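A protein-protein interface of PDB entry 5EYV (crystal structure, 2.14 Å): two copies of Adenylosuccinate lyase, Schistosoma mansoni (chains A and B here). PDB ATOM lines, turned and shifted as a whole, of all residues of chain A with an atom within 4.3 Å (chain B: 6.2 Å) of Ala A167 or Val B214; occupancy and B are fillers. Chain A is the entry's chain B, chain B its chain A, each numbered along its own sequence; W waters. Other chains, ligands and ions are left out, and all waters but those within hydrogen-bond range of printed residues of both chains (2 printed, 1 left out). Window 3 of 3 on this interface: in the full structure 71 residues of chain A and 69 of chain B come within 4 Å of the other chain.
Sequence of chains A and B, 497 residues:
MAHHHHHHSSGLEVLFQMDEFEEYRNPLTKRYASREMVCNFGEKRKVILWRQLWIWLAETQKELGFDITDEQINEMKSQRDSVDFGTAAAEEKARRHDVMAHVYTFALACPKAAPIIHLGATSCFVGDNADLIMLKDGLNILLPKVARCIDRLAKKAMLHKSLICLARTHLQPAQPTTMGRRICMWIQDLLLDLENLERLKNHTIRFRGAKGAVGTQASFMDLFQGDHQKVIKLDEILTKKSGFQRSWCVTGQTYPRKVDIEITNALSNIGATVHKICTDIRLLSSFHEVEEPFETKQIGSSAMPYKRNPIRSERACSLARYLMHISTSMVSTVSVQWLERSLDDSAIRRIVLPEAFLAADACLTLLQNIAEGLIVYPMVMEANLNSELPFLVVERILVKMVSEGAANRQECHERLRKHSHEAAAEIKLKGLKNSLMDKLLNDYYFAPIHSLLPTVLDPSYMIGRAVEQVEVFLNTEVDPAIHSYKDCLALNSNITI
Leu A166 touches none of the printed residues of chain B. Of the printed residues of chain B, Ala A167 touches Val B214 (3.6 Å) and Glu B340 (3.5 Å). Of the printed residues of chain B, Gln A175 touches Ala B213, Val B214 and Thr B216. Of the printed residues of chain B, Arg A182 touches Glu B340 (2.6 Å). Gln B217 touches none of the printed residues of chain A. The nearest printed residue of chain A that does not touch Glu B340 is Thr A169 (4.2 Å).
OE1 of Glu B340 lies within salt-bridge range of NH2 of Arg A182, at 2.6 Å. The side-chain carboxylate (OE1) of Glu B340 lies within hydrogen-bond range of the backbone NH (N) of Arg A168, 3.0 Å away.
The side-chain amide oxygen of Gln B253 sits close to the backbone carbonyl oxygen of Ala B213, 2.8 Å away. N of Gln B253 sits at hydrogen-bond distance from O of Glu B340. The backbone carbonyl oxygen of Thr A177 lies within hydrogen-bond range of the backbone NH of Cys A165, 2.7 Å away. The backbone carbonyl oxygen (O) of Ala A167 sits at hydrogen-bond distance from the backbone NH (N) of Ala A174, at 2.7 Å. The backbone carbonyl oxygen (O) of Lys B211 is in hydrogen-bond range of the backbone NH (N) of Thr B216. NH2 of Arg A182 sits at hydrogen-bond distance from O of Leu A166, 2.9 Å away.
Among the printed residues, merely in contact across the chains: Ala A167 with Val B214, Ala A167 with Glu B340, Gln A175 with Ala B213, Gln A175 with Val B214, Gln A175 with Thr B216 and Thr A177 with Thr B216.
Water W1 lies within hydrogen-bond range of the side-chain amide nitrogen (NE2) of Gln A175 (2.7 Å) and the backbone NH (N) of Ala B213 (3.3 Å). Water W2 bridges OG1 of Thr A177 (2.7 Å) and O of Val B214 (3.3 Å).
Of the 12 printed residues of chain A, 5 touch a printed residue of chain B. Of the 12 printed residues of chain B, 4 touch a printed residue of chain A. Printed residues of chain B that touch a printed residue of chain A: Ala B213, Val B214, Thr B216 and Glu B340. Among the printed residues, Asp or Glu carboxylates within 4 Å of a Lys or Arg side-chain nitrogen of the other chain: Arg A182 with Glu B340.
No position is printed for both chains.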
ATOM      1  N   CYS A 165       0.665 -29.686 -11.741  1.00  0.00           N
ATOM      2  CA  CYS A 165       1.819 -29.334 -10.930  1.00  0.00           C
ATOM      3  C   CYS A 165       1.353 -29.083  -9.502  1.00  0.00           C
ATOM      4  O   CYS A 165       0.158 -29.123  -9.198  1.00  0.00           O
ATOM      5  CB  CYS A 165       2.549 -28.115 -11.500  1.00  0.00           C
ATOM      6  SG  CYS A 165       1.655 -26.554 -11.322  1.00  0.00           S
ATOM      7  N   LEU A 166       2.315 -28.817  -8.626  1.00  0.00           N
ATOM      8  CA  LEU A 166       2.043 -28.608  -7.213  1.00  0.00           C
ATOM      9  C   LEU A 166       1.813 -27.127  -6.940  1.00  0.00           C
ATOM     10  O   LEU A 166       2.646 -26.287  -7.298  1.00  0.00           O
ATOM     11  CB  LEU A 166       3.205 -29.135  -6.371  1.00  0.00           C
ATOM     12  CG  LEU A 166       2.999 -29.367  -4.875  1.00  0.00           C
ATOM     13  CD1 LEU A 166       1.785 -30.241  -4.626  1.00  0.00           C
ATOM     14  CD2 LEU A 166       4.243 -30.011  -4.288  1.00  0.00           C
ATOM     15  N   ALA A 167       0.679 -26.811  -6.322  1.00  0.00           N
ATOM     16  CA  ALA A 167       0.417 -25.466  -5.835  1.00  0.00           C
ATOM     17  C   ALA A 167       0.995 -25.310  -4.435  1.00  0.00           C
ATOM     18  O   ALA A 167       1.021 -26.255  -3.644  1.00  0.00           O
ATOM     19  CB  ALA A 167      -1.081 -25.167  -5.818  1.00  0.00           C
ATOM     20  N   ARG A 168       1.462 -24.101  -4.133  1.00  0.00           N
ATOM     21  CA  ARG A 168       2.154 -23.833  -2.879  1.00  0.00           C
ATOM     22  C   ARG A 168       1.504 -22.655  -2.169  1.00  0.00           C
ATOM     23  O   ARG A 168       1.448 -21.549  -2.715  1.00  0.00           O
ATOM     24  CB  ARG A 168       3.641 -23.556  -3.118  1.00  0.00           C
ATOM     25  CG  ARG A 168       4.486 -24.809  -3.263  1.00  0.00           C
ATOM     26  CD  ARG A 168       5.222 -24.834  -4.591  1.00  0.00           C
ATOM     27  NE  ARG A 168       6.117 -25.983  -4.687  1.00  0.00           N
ATOM     28  CZ  ARG A 168       6.730 -26.363  -5.804  1.00  0.00           C
ATOM     29  NH1 ARG A 168       6.543 -25.689  -6.929  1.00  0.00           N
ATOM     30  NH2 ARG A 168       7.528 -27.423  -5.796  1.00  0.00           N
ATOM     31  N   THR A 169       1.013 -22.901  -0.958  1.00  0.00           N
ATOM     32  CA  THR A 169       0.621 -21.855  -0.027  1.00  0.00           C
ATOM     33  C   THR A 169       1.583 -21.880   1.154  1.00  0.00           C
ATOM     34  O   THR A 169       1.937 -22.954   1.652  1.00  0.00           O
ATOM     35  CB  THR A 169      -0.822 -22.040   0.452  1.00  0.00           C
ATOM     36  OG1 THR A 169      -0.980 -23.346   1.019  1.00  0.00           O
ATOM     37  CG2 THR A 169      -1.792 -21.878  -0.711  1.00  0.00           C
ATOM     38  N   GLN A 172       4.646 -24.011   0.903  1.00  0.00           N
ATOM     39  CA  GLN A 172       4.596 -25.428   1.221  1.00  0.00           C
ATOM     40  C   GLN A 172       3.562 -26.116   0.338  1.00  0.00           C
ATOM     41  O   GLN A 172       2.613 -25.474  -0.122  1.00  0.00           O
ATOM     42  CB  GLN A 172       4.251 -25.655   2.699  1.00  0.00           C
ATOM     43  CG  GLN A 172       5.352 -25.238   3.669  1.00  0.00           C
ATOM     44  CD  GLN A 172       6.259 -26.387   4.066  1.00  0.00           C
ATOM     45  OE1 GLN A 172       5.949 -27.554   3.825  1.00  0.00           O
ATOM     46  NE2 GLN A 172       7.388 -26.061   4.685  1.00  0.00           N
ATOM     47  N   PRO A 173       3.725 -27.412   0.073  1.00  0.00           N
ATOM     48  CA  PRO A 173       2.831 -28.095  -0.873  1.00  0.00           C
ATOM     49  C   PRO A 173       1.368 -28.003  -0.459  1.00  0.00           C
ATOM     50  O   PRO A 173       1.004 -28.295   0.682  1.00  0.00           O
ATOM     51  CB  PRO A 173       3.334 -29.542  -0.845  1.00  0.00           C
ATOM     52  CG  PRO A 173       4.765 -29.422  -0.467  1.00  0.00           C
ATOM     53  CD  PRO A 173       4.831 -28.283   0.506  1.00  0.00           C
ATOM     54  N   ALA A 174       0.534 -27.590  -1.407  1.00  0.00           N
ATOM     55  CA  ALA A 174      -0.912 -27.534  -1.254  1.00  0.00           C
ATOM     56  C   ALA A 174      -1.554 -28.400  -2.339  1.00  0.00           C
ATOM     57  O   ALA A 174      -0.867 -29.102  -3.084  1.00  0.00           O
ATOM     58  CB  ALA A 174      -1.404 -26.085  -1.307  1.00  0.00           C
ATOM     59  N   GLN A 175      -2.882 -28.342  -2.425  1.00  0.00           N
ATOM     60  CA  GLN A 175      -3.605 -29.187  -3.363  1.00  0.00           C
ATOM     61  C   GLN A 175      -3.189 -28.869  -4.801  1.00  0.00           C
ATOM     62  O   GLN A 175      -2.828 -27.732  -5.115  1.00  0.00           O
ATOM     63  CB  GLN A 175      -5.113 -29.005  -3.188  1.00  0.00           C
ATOM     64  CG  GLN A 175      -5.602 -27.583  -3.373  1.00  0.00           C
ATOM     65  CD  GLN A 175      -7.047 -27.412  -2.951  1.00  0.00           C
ATOM     66  OE1 GLN A 175      -7.394 -27.615  -1.787  1.00  0.00           O
ATOM     67  NE2 GLN A 175      -7.901 -27.041  -3.899  1.00  0.00           N
ATOM     68  N   PRO A 176      -3.224 -29.859  -5.692  1.00  0.00           N
ATOM     69  CA  PRO A 176      -2.642 -29.677  -7.027  1.00  0.00           C
ATOM     70  C   PRO A 176      -3.378 -28.638  -7.862  1.00  0.00           C
ATOM     71  O   PRO A 176      -4.535 -28.290  -7.614  1.00  0.00           O
ATOM     72  CB  PRO A 176      -2.758 -31.069  -7.659  1.00  0.00           C
ATOM     73  CG  PRO A 176      -2.878 -32.007  -6.501  1.00  0.00           C
ATOM     74  CD  PRO A 176      -3.650 -31.251  -5.466  1.00  0.00           C
ATOM     75  N   THR A 177      -2.665 -28.143  -8.870  1.00  0.00           N
ATOM     76  CA  THR A 177      -3.202 -27.237  -9.877  1.00  0.00           C
ATOM     77  C   THR A 177      -2.446 -27.496 -11.177  1.00  0.00           C
ATOM     78  O   THR A 177      -1.646 -28.431 -11.271  1.00  0.00           O
ATOM     79  CB  THR A 177      -3.088 -25.775  -9.421  1.00  0.00           C
ATOM     80  OG1 THR A 177      -3.794 -24.928 -10.337  1.00  0.00           O
ATOM     81  CG2 THR A 177      -1.629 -25.343  -9.371  1.00  0.00           C
ATOM     82  N   ARG A 182      -1.815 -21.298 -13.109  1.00  0.00           N
ATOM     83  CA  ARG A 182      -0.978 -20.372 -12.357  1.00  0.00           C
ATOM     84  C   ARG A 182      -0.508 -19.211 -13.226  1.00  0.00           C
ATOM     85  O   ARG A 182      -0.401 -18.077 -12.748  1.00  0.00           O
ATOM     86  CB  ARG A 182       0.218 -21.121 -11.767  1.00  0.00           C
ATOM     87  CG  ARG A 182       1.334 -20.230 -11.247  1.00  0.00           C
ATOM     88  CD  ARG A 182       2.484 -21.071 -10.728  1.00  0.00           C
ATOM     89  NE  ARG A 182       2.115 -21.805  -9.522  1.00  0.00           N
ATOM     90  CZ  ARG A 182       2.664 -22.957  -9.153  1.00  0.00           C
ATOM     91  NH1 ARG A 182       3.598 -23.519  -9.907  1.00  0.00           N
ATOM     92  NH2 ARG A 182       2.270 -23.555  -8.037  1.00  0.00           N
ATOM     93  N   ARG B 208     -14.545 -11.889  -4.303  1.00  0.00           N
ATOM     94  CA  ARG B 208     -13.670 -13.055  -4.297  1.00  0.00           C
ATOM     95  C   ARG B 208     -14.439 -14.349  -4.522  1.00  0.00           C
ATOM     96  O   ARG B 208     -13.914 -15.271  -5.157  1.00  0.00           O
ATOM     97  CB  ARG B 208     -12.893 -13.124  -2.978  1.00  0.00           C
ATOM     98  CG  ARG B 208     -11.817 -14.205  -2.915  1.00  0.00           C
ATOM     99  CD  ARG B 208     -12.302 -15.445  -2.176  1.00  0.00           C
ATOM    100  NE  ARG B 208     -11.276 -16.481  -2.100  1.00  0.00           N
ATOM    101  CZ  ARG B 208     -11.501 -17.722  -1.679  1.00  0.00           C
ATOM    102  NH1 ARG B 208     -12.718 -18.085  -1.298  1.00  0.00           N
ATOM    103  NH2 ARG B 208     -10.509 -18.602  -1.642  1.00  0.00           N
ATOM    104  N   LYS B 211     -13.716 -20.049  -4.288  1.00  0.00           N
ATOM    105  CA  LYS B 211     -12.678 -20.492  -5.209  1.00  0.00           C
ATOM    106  C   LYS B 211     -11.865 -21.682  -4.727  1.00  0.00           C
ATOM    107  O   LYS B 211     -11.161 -22.286  -5.544  1.00  0.00           O
ATOM    108  CB  LYS B 211     -11.711 -19.340  -5.521  1.00  0.00           C
ATOM    109  CG  LYS B 211     -12.317 -18.236  -6.361  1.00  0.00           C
ATOM    110  CD  LYS B 211     -12.910 -18.794  -7.642  1.00  0.00           C
ATOM    111  CE  LYS B 211     -13.477 -17.683  -8.507  1.00  0.00           C
ATOM    112  NZ  LYS B 211     -14.329 -18.201  -9.611  1.00  0.00           N
ATOM    113  N   GLY B 212     -11.926 -22.038  -3.452  1.00  0.00           N
ATOM    114  CA  GLY B 212     -11.118 -23.122  -2.933  1.00  0.00           C
ATOM    115  C   GLY B 212      -9.826 -22.625  -2.317  1.00  0.00           C
ATOM    116  O   GLY B 212      -9.620 -21.432  -2.076  1.00  0.00           O
ATOM    117  N   ALA B 213      -8.929 -23.582  -2.067  1.00  0.00           N
ATOM    118  CA  ALA B 213      -7.665 -23.261  -1.415  1.00  0.00           C
ATOM    119  C   ALA B 213      -6.667 -22.611  -2.366  1.00  0.00           C
ATOM    120  O   ALA B 213      -5.847 -21.799  -1.930  1.00  0.00           O
ATOM    121  CB  ALA B 213      -7.054 -24.522  -0.802  1.00  0.00           C
ATOM    122  N   VAL B 214      -6.709 -22.954  -3.654  1.00  0.00           N
ATOM    123  CA  VAL B 214      -5.754 -22.410  -4.613  1.00  0.00           C
ATOM    124  C   VAL B 214      -6.491 -21.853  -5.823  1.00  0.00           C
ATOM    125  O   VAL B 214      -5.910 -21.702  -6.903  1.00  0.00           O
ATOM    126  CB  VAL B 214      -4.722 -23.473  -5.036  1.00  0.00           C
ATOM    127  CG1 VAL B 214      -3.849 -23.870  -3.853  1.00  0.00           C
ATOM    128  CG2 VAL B 214      -5.420 -24.690  -5.621  1.00  0.00           C
ATOM    129  N   GLY B 215      -7.774 -21.544  -5.651  1.00  0.00           N
ATOM    130  CA  GLY B 215      -8.549 -20.907  -6.697  1.00  0.00           C
ATOM    131  C   GLY B 215      -9.067 -21.822  -7.783  1.00  0.00           C
ATOM    132  O   GLY B 215      -9.645 -21.327  -8.757  1.00  0.00           O
ATOM    133  N   THR B 216      -8.889 -23.134  -7.652  1.00  0.00           N
ATOM    134  CA  THR B 216      -9.325 -24.074  -8.675  1.00  0.00           C
ATOM    135  C   THR B 216     -10.720 -24.629  -8.422  1.00  0.00           C
ATOM    136  O   THR B 216     -11.225 -25.387  -9.257  1.00  0.00           O
ATOM    137  CB  THR B 216      -8.334 -25.236  -8.789  1.00  0.00           C
ATOM    138  OG1 THR B 216      -8.352 -26.005  -7.580  1.00  0.00           O
ATOM    139  CG2 THR B 216      -6.927 -24.714  -9.031  1.00  0.00           C
ATOM    140  N   GLN B 217     -11.350 -24.274  -7.301  1.00  0.00           N
ATOM    141  CA  GLN B 217     -12.683 -24.767  -6.949  1.00  0.00           C
ATOM    142  C   GLN B 217     -12.737 -26.292  -6.932  1.00  0.00           C
ATOM    143  O   GLN B 217     -13.785 -26.890  -7.187  1.00  0.00           O
ATOM    144  CB  GLN B 217     -13.750 -24.205  -7.893  1.00  0.00           C
ATOM    145  CG  GLN B 217     -13.909 -22.696  -7.824  1.00  0.00           C
ATOM    146  CD  GLN B 217     -14.716 -22.142  -8.980  1.00  0.00           C
ATOM    147  OE1 GLN B 217     -14.383 -22.360 -10.146  1.00  0.00           O
ATOM    148  NE2 GLN B 217     -15.786 -21.423  -8.664  1.00  0.00           N
ATOM    149  N   THR B 251      -8.061 -16.415  -9.513  1.00  0.00           N
ATOM    150  CA  THR B 251      -7.318 -16.100  -8.304  1.00  0.00           C
ATOM    151  C   THR B 251      -6.414 -17.261  -7.906  1.00  0.00           C
ATOM    152  O   THR B 251      -6.539 -18.388  -8.394  1.00  0.00           O
ATOM    153  CB  THR B 251      -8.260 -15.795  -7.141  1.00  0.00           C
ATOM    154  OG1 THR B 251      -9.066 -16.946  -6.861  1.00  0.00           O
ATOM    155  CG2 THR B 251      -9.150 -14.628  -7.462  1.00  0.00           C
ATOM    156  N   GLY B 252      -5.491 -16.968  -6.999  1.00  0.00           N
ATOM    157  CA  GLY B 252      -4.830 -18.013  -6.251  1.00  0.00           C
ATOM    158  C   GLY B 252      -5.687 -18.360  -5.052  1.00  0.00           C
ATOM    159  O   GLY B 252      -6.845 -18.756  -5.206  1.00  0.00           O
ATOM    160  N   GLN B 253      -5.140 -18.186  -3.849  1.00  0.00           N
ATOM    161  CA  GLN B 253      -5.930 -18.399  -2.642  1.00  0.00           C
ATOM    162  C   GLN B 253      -6.852 -17.217  -2.365  1.00  0.00           C
ATOM    163  O   GLN B 253      -8.038 -17.399  -2.068  1.00  0.00           O
ATOM    164  CB  GLN B 253      -5.004 -18.649  -1.450  1.00  0.00           C
ATOM    165  CG  GLN B 253      -5.685 -18.562  -0.096  1.00  0.00           C
ATOM    166  CD  GLN B 253      -6.424 -19.829   0.281  1.00  0.00           C
ATOM    167  OE1 GLN B 253      -5.812 -20.820   0.683  1.00  0.00           O
ATOM    168  NE2 GLN B 253      -7.744 -19.804   0.156  1.00  0.00           N
ATOM    169  N   GLU B 340       0.907 -19.223  -5.055  1.00  0.00           N
ATOM    170  CA  GLU B 340      -0.529 -19.272  -4.805  1.00  0.00           C
ATOM    171  C   GLU B 340      -0.924 -18.456  -3.582  1.00  0.00           C
ATOM    172  O   GLU B 340      -2.036 -17.914  -3.543  1.00  0.00           O
ATOM    173  CB  GLU B 340      -0.992 -20.722  -4.666  1.00  0.00           C
ATOM    174  CG  GLU B 340      -1.202 -21.428  -6.001  1.00  0.00           C
ATOM    175  CD  GLU B 340       0.070 -21.534  -6.821  1.00  0.00           C
ATOM    176  OE1 GLU B 340       1.084 -22.034  -6.291  1.00  0.00           O
ATOM    177  OE2 GLU B 340       0.062 -21.104  -7.993  1.00  0.00           O
HETATM  178  O   HOH W   1     -10.337 -26.379  -3.027  1.00  0.00           O
HETATM  179  O   HOH W   2      -3.561 -22.532  -9.068  1.00  0.00           O
